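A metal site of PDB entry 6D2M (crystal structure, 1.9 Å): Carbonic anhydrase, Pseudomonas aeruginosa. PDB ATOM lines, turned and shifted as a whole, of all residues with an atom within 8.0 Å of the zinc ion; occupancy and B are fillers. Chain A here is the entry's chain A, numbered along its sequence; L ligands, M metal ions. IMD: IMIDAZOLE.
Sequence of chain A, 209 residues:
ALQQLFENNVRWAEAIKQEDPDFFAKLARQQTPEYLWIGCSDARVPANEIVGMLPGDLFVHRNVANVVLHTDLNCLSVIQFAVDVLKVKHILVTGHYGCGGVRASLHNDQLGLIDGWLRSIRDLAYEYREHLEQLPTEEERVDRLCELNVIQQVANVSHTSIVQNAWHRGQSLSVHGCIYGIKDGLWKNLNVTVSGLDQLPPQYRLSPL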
ATOM      1  N   GLY A  39     -14.931  19.014 -17.425  1.00  0.00           N
ATOM      2  CA  GLY A  39     -15.879  19.688 -18.269  1.00  0.00           C
ATOM      3  C   GLY A  39     -16.271  18.888 -19.476  1.00  0.00           C
ATOM      4  O   GLY A  39     -15.915  17.731 -19.610  1.00  0.00           O
ATOM      5  N   CYS A  40     -17.016  19.520 -20.367  1.00  0.00           N
ATOM      6  CA  CYS A  40     -17.479  18.837 -21.561  1.00  0.00           C
ATOM      7  C   CYS A  40     -16.425  18.930 -22.667  1.00  0.00           C
ATOM      8  O   CYS A  40     -15.617  19.880 -22.682  1.00  0.00           O
ATOM      9  CB  CYS A  40     -18.817  19.432 -22.024  1.00  0.00           C
ATOM     10  SG  CYS A  40     -19.543  18.587 -23.451  1.00  0.00           S
ATOM     11  N   SER A  41     -16.454  17.948 -23.557  1.00  0.00           N
ATOM     12  CA  SER A  41     -15.590  17.903 -24.743  1.00  0.00           C
ATOM     13  C   SER A  41     -15.888  18.983 -25.775  1.00  0.00           C
ATOM     14  O   SER A  41     -15.059  19.283 -26.642  1.00  0.00           O
ATOM     15  CB  SER A  41     -15.721  16.514 -25.404  1.00  0.00           C
ATOM     16  OG  SER A  41     -15.132  15.509 -24.568  1.00  0.00           O
ATOM     17  N   ASP A  42     -17.110  19.531 -25.700  1.00  0.00           N
ATOM     18  CA  ASP A  42     -17.602  20.560 -26.606  1.00  0.00           C
ATOM     19  C   ASP A  42     -16.491  21.544 -26.961  1.00  0.00           C
ATOM     20  O   ASP A  42     -15.844  22.093 -26.077  1.00  0.00           O
ATOM     21  CB  ASP A  42     -18.785  21.293 -25.959  1.00  0.00           C
ATOM     22  CG  ASP A  42     -19.513  22.213 -26.942  1.00  0.00           C
ATOM     23  OD1 ASP A  42     -20.760  22.126 -27.033  1.00  0.00           O
ATOM     24  OD2 ASP A  42     -18.829  23.007 -27.619  1.00  0.00           O
ATOM     25  N   ALA A  43     -16.262  21.732 -28.261  1.00  0.00           N
ATOM     26  CA  ALA A  43     -15.130  22.519 -28.759  1.00  0.00           C
ATOM     27  C   ALA A  43     -15.200  23.979 -28.319  1.00  0.00           C
ATOM     28  O   ALA A  43     -14.210  24.699 -28.384  1.00  0.00           O
ATOM     29  CB  ALA A  43     -15.061  22.436 -30.279  1.00  0.00           C
ATOM     30  N   ARG A  44     -16.380  24.394 -27.892  1.00  0.00           N
ATOM     31  CA  ARG A  44     -16.625  25.784 -27.545  1.00  0.00           C
ATOM     32  C   ARG A  44     -16.333  26.051 -26.082  1.00  0.00           C
ATOM     33  O   ARG A  44     -16.518  27.181 -25.595  1.00  0.00           O
ATOM     34  CB  ARG A  44     -18.063  26.162 -27.881  1.00  0.00           C
ATOM     35  CG  ARG A  44     -18.337  26.142 -29.377  1.00  0.00           C
ATOM     36  CD  ARG A  44     -19.825  26.133 -29.678  1.00  0.00           C
ATOM     37  NE  ARG A  44     -20.492  24.949 -29.133  1.00  0.00           N
ATOM     38  CZ  ARG A  44     -21.750  24.631 -29.416  1.00  0.00           C
ATOM     39  NH1 ARG A  44     -22.450  25.397 -30.235  1.00  0.00           N
ATOM     40  NH2 ARG A  44     -22.308  23.548 -28.881  1.00  0.00           N
ATOM     41  N   VAL A  45     -15.853  25.024 -25.354  1.00  0.00           N
ATOM     42  CA  VAL A  45     -15.613  25.203 -23.927  1.00  0.00           C
ATOM     43  C   VAL A  45     -14.198  24.796 -23.518  1.00  0.00           C
ATOM     44  O   VAL A  45     -14.017  23.927 -22.682  1.00  0.00           O
ATOM     45  CB  VAL A  45     -16.645  24.402 -23.081  1.00  0.00           C
ATOM     46  CG1 VAL A  45     -16.720  24.955 -21.660  1.00  0.00           C
ATOM     47  CG2 VAL A  45     -18.038  24.458 -23.719  1.00  0.00           C
ATOM     48  N   ASN A  63     -15.080  15.126 -21.187  1.00  0.00           N
ATOM     49  CA  ASN A  63     -15.833  14.026 -21.765  1.00  0.00           C
ATOM     50  C   ASN A  63     -17.201  14.539 -22.206  1.00  0.00           C
ATOM     51  O   ASN A  63     -17.515  15.704 -21.982  1.00  0.00           O
ATOM     52  CB  ASN A  63     -15.939  12.831 -20.770  1.00  0.00           C
ATOM     53  CG  ASN A  63     -16.835  13.117 -19.542  1.00  0.00           C
ATOM     54  OD1 ASN A  63     -17.936  13.626 -19.663  1.00  0.00           O
ATOM     55  ND2 ASN A  63     -16.348  12.718 -18.360  1.00  0.00           N
ATOM     56  N   VAL A  64     -18.023  13.694 -22.825  1.00  0.00           N
ATOM     57  CA  VAL A  64     -19.318  14.157 -23.271  1.00  0.00           C
ATOM     58  C   VAL A  64     -20.245  14.476 -22.085  1.00  0.00           C
ATOM     59  O   VAL A  64     -20.616  13.608 -21.297  1.00  0.00           O
ATOM     60  CB  VAL A  64     -20.013  13.125 -24.187  1.00  0.00           C
ATOM     61  CG1 VAL A  64     -21.375  13.651 -24.609  1.00  0.00           C
ATOM     62  CG2 VAL A  64     -19.152  12.851 -25.419  1.00  0.00           C
ATOM     63  N   ALA A  65     -20.604  15.745 -21.989  1.00  0.00           N
ATOM     64  CA  ALA A  65     -21.504  16.276 -20.966  1.00  0.00           C
ATOM     65  C   ALA A  65     -20.964  16.168 -19.550  1.00  0.00           C
ATOM     66  O   ALA A  65     -21.733  16.172 -18.603  1.00  0.00           O
ATOM     67  CB  ALA A  65     -22.874  15.603 -21.041  1.00  0.00           C
ATOM     68  N   ASN A  66     -19.635  16.162 -19.409  1.00  0.00           N
ATOM     69  CA  ASN A  66     -18.961  16.218 -18.102  1.00  0.00           C
ATOM     70  C   ASN A  66     -19.600  15.322 -17.076  1.00  0.00           C
ATOM     71  O   ASN A  66     -20.025  15.770 -16.002  1.00  0.00           O
ATOM     72  CB  ASN A  66     -18.896  17.665 -17.566  1.00  0.00           C
ATOM     73  CG  ASN A  66     -20.221  18.438 -17.697  1.00  0.00           C
ATOM     74  OD1 ASN A  66     -20.507  19.030 -18.738  1.00  0.00           O
ATOM     75  ND2 ASN A  66     -21.005  18.447 -16.625  1.00  0.00           N
ATOM     76  N   THR A  94     -17.336  21.994 -14.497  1.00  0.00           N
ATOM     77  CA  THR A  94     -17.935  22.998 -15.350  1.00  0.00           C
ATOM     78  C   THR A  94     -18.740  22.379 -16.475  1.00  0.00           C
ATOM     79  O   THR A  94     -18.195  21.734 -17.379  1.00  0.00           O
ATOM     80  CB  THR A  94     -16.864  23.938 -15.981  1.00  0.00           C
ATOM     81  OG1 THR A  94     -16.053  24.512 -14.939  1.00  0.00           O
ATOM     82  CG2 THR A  94     -17.529  25.046 -16.778  1.00  0.00           C
ATOM     83  N   GLY A  95     -20.053  22.563 -16.412  1.00  0.00           N
ATOM     84  CA  GLY A  95     -20.912  22.187 -17.517  1.00  0.00           C
ATOM     85  C   GLY A  95     -21.104  23.432 -18.352  1.00  0.00           C
ATOM     86  O   GLY A  95     -20.481  24.463 -18.100  1.00  0.00           O
ATOM     87  N   HIS A  96     -21.947  23.345 -19.374  1.00  0.00           N
ATOM     88  CA  HIS A  96     -22.268  24.547 -20.132  1.00  0.00           C
ATOM     89  C   HIS A  96     -23.706  24.503 -20.623  1.00  0.00           C
ATOM     90  O   HIS A  96     -24.315  23.438 -20.731  1.00  0.00           O
ATOM     91  CB  HIS A  96     -21.303  24.709 -21.304  1.00  0.00           C
ATOM     92  CG  HIS A  96     -21.390  23.616 -22.329  1.00  0.00           C
ATOM     93  ND1 HIS A  96     -22.048  23.767 -23.527  1.00  0.00           N
ATOM     94  CD2 HIS A  96     -20.903  22.351 -22.314  1.00  0.00           C
ATOM     95  CE1 HIS A  96     -21.952  22.639 -24.217  1.00  0.00           C
ATOM     96  NE2 HIS A  96     -21.262  21.773 -23.504  1.00  0.00           N
ATOM     97  N   TYR A  97     -24.259  25.685 -20.885  1.00  0.00           N
ATOM     98  CA  TYR A  97     -25.586  25.778 -21.459  1.00  0.00           C
ATOM     99  C   TYR A  97     -25.564  25.302 -22.911  1.00  0.00           C
ATOM    100  O   TYR A  97     -24.526  25.330 -23.564  1.00  0.00           O
ATOM    101  CB  TYR A  97     -26.106  27.220 -21.382  1.00  0.00           C
ATOM    102  CG  TYR A  97     -26.407  27.679 -19.963  1.00  0.00           C
ATOM    103  CD1 TYR A  97     -25.736  28.751 -19.394  1.00  0.00           C
ATOM    104  CD2 TYR A  97     -27.375  27.029 -19.208  1.00  0.00           C
ATOM    105  CE1 TYR A  97     -26.025  29.156 -18.085  1.00  0.00           C
ATOM    106  CE2 TYR A  97     -27.666  27.429 -17.920  1.00  0.00           C
ATOM    107  CZ  TYR A  97     -26.995  28.488 -17.362  1.00  0.00           C
ATOM    108  OH  TYR A  97     -27.312  28.854 -16.070  1.00  0.00           O
ATOM    109  N   GLY A  98     -26.714  24.859 -23.402  1.00  0.00           N
ATOM    110  CA  GLY A  98     -26.816  24.376 -24.758  1.00  0.00           C
ATOM    111  C   GLY A  98     -26.053  23.086 -25.008  1.00  0.00           C
ATOM    112  O   GLY A  98     -25.729  22.757 -26.144  1.00  0.00           O
ATOM    113  N   CYS A  99     -25.763  22.346 -23.939  1.00  0.00           N
ATOM    114  CA  CYS A  99     -24.993  21.098 -24.102  1.00  0.00           C
ATOM    115  C   CYS A  99     -25.766  20.058 -24.903  1.00  0.00           C
ATOM    116  O   CYS A  99     -26.855  19.653 -24.516  1.00  0.00           O
ATOM    117  CB  CYS A  99     -24.595  20.524 -22.744  1.00  0.00           C
ATOM    118  SG  CYS A  99     -23.526  19.048 -22.862  1.00  0.00           S
ATOM    119  N   GLY A 100     -25.173  19.615 -26.016  1.00  0.00           N
ATOM    120  CA  GLY A 100     -25.812  18.632 -26.875  1.00  0.00           C
ATOM    121  C   GLY A 100     -25.951  17.257 -26.247  1.00  0.00           C
ATOM    122  O   GLY A 100     -26.885  16.512 -26.549  1.00  0.00           O
ATOM    123  N   GLY A 101     -24.999  16.893 -25.384  1.00  0.00           N
ATOM    124  CA  GLY A 101     -25.080  15.648 -24.633  1.00  0.00           C
ATOM    125  C   GLY A 101     -26.294  15.674 -23.718  1.00  0.00           C
ATOM    126  O   GLY A 101     -27.057  14.700 -23.646  1.00  0.00           O
ATOM    127  N   VAL A 102     -26.470  16.780 -23.015  1.00  0.00           N
ATOM    128  CA  VAL A 102     -27.623  16.975 -22.165  1.00  0.00           C
ATOM    129  C   VAL A 102     -28.904  16.983 -23.006  1.00  0.00           C
ATOM    130  O   VAL A 102     -29.881  16.316 -22.673  1.00  0.00           O
ATOM    131  CB  VAL A 102     -27.511  18.279 -21.350  1.00  0.00           C
ATOM    132  CG1 VAL A 102     -28.765  18.513 -20.536  1.00  0.00           C
ATOM    133  CG2 VAL A 102     -26.280  18.219 -20.443  1.00  0.00           C
ATOM    134  N   ARG A 103     -28.890  17.724 -24.113  1.00  0.00           N
ATOM    135  CA  ARG A 103     -30.056  17.802 -24.988  1.00  0.00           C
ATOM    136  C   ARG A 103     -30.471  16.410 -25.461  1.00  0.00           C
ATOM    137  O   ARG A 103     -31.659  16.063 -25.459  1.00  0.00           O
ATOM    138  CB  ARG A 103     -29.769  18.693 -26.191  1.00  0.00           C
ATOM    139  CG  ARG A 103     -30.906  18.753 -27.222  1.00  0.00           C
ATOM    140  CD  ARG A 103     -30.722  19.899 -28.214  1.00  0.00           C
ATOM    141  NE  ARG A 103     -31.326  21.147 -27.731  1.00  0.00           N
ATOM    142  CZ  ARG A 103     -30.656  22.235 -27.359  1.00  0.00           C
ATOM    143  NH1 ARG A 103     -29.328  22.277 -27.417  1.00  0.00           N
ATOM    144  NH2 ARG A 103     -31.326  23.304 -26.946  1.00  0.00           N
ATOM    145  N   CYS A 146     -28.954  21.216 -17.787  1.00  0.00           N
ATOM    146  CA  CYS A 146     -27.515  21.457 -17.804  1.00  0.00           C
ATOM    147  C   CYS A 146     -27.018  21.831 -16.406  1.00  0.00           C
ATOM    148  O   CYS A 146     -25.978  21.374 -15.951  1.00  0.00           O
ATOM    149  CB  CYS A 146     -27.143  22.570 -18.788  1.00  0.00           C
ATOM    150  SG  CYS A 146     -27.144  22.041 -20.525  1.00  0.00           S
ATOM    151  N   ASN A 149     -27.460  18.897 -13.957  1.00  0.00           N
ATOM    152  CA  ASN A 149     -26.380  17.940 -14.209  1.00  0.00           C
ATOM    153  C   ASN A 149     -25.094  18.339 -13.482  1.00  0.00           C
ATOM    154  O   ASN A 149     -24.520  17.520 -12.750  1.00  0.00           O
ATOM    155  CB  ASN A 149     -26.095  17.807 -15.702  1.00  0.00           C
ATOM    156  CG  ASN A 149     -25.101  16.706 -16.001  1.00  0.00           C
ATOM    157  OD1 ASN A 149     -25.127  15.643 -15.360  1.00  0.00           O
ATOM    158  ND2 ASN A 149     -24.195  16.947 -16.946  1.00  0.00           N
ATOM    159  N   ILE A 182     -22.092  29.396 -23.634  1.00  0.00           N
ATOM    160  CA  ILE A 182     -21.465  29.447 -24.952  1.00  0.00           C
ATOM    161  C   ILE A 182     -21.973  30.673 -25.706  1.00  0.00           C
ATOM    162  O   ILE A 182     -21.366  31.124 -26.682  1.00  0.00           O
ATOM    163  CB  ILE A 182     -21.725  28.170 -25.786  1.00  0.00           C
ATOM    164  CG1 ILE A 182     -23.219  27.808 -25.803  1.00  0.00           C
ATOM    165  CG2 ILE A 182     -20.915  27.001 -25.235  1.00  0.00           C
ATOM    166  CD1 ILE A 182     -23.591  26.537 -26.642  1.00  0.00           C
HETATM  167  N1  IMD L   1     -21.689  19.074 -25.951  1.00  0.00           N
HETATM  168  C2  IMD L   1     -21.921  19.279 -27.239  1.00  0.00           C
HETATM  169  N3  IMD L   1     -21.986  18.122 -27.879  1.00  0.00           N
HETATM  170  C4  IMD L   1     -21.800  17.119 -27.005  1.00  0.00           C
HETATM  171  C5  IMD L   1     -21.619  17.732 -25.759  1.00  0.00           C
HETATM  172 ZN    ZN M   1     -21.485  19.691 -23.885  1.00  0.00          ZN
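CB of Asp 42 touches the zinc ion, at 3.8 Å.
The nearest printed residue that does not touch the zinc ion is Gly 100 (4.3 Å).
The zinc ion is bound by a ring nitrogen (NE2) of His 96 (2.1 Å), a nitrogen (N1) of the ligand (2.2 Å), the side-chain sulfur of Cys 40 (2.3 Å) and the side-chain sulfur of Cys 99 (2.4 Å).
O of His 96 lies within hydrogen-bond range of SG of Cys 146 (3.2 Å).
The side-chain sulfur (SG) of Cys 40 sits close to the backbone NH (N) of Asp 42 (3.4 Å).
SG of Cys 40 sits close to N of Ala 65 (3.4 Å).
The side-chain sulfur (SG) of Cys 99 sits close to the backbone NH (N) of Gly 101 (3.6 Å).
SG of Cys 99 lies close to N of Val 102 (3.7 Å).
N of Cys 99 sits at hydrogen-bond distance from SG of Cys 146 (3.7 Å).
OD1 of Asp 42 is in salt-bridge range of NH2 of Arg 44.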
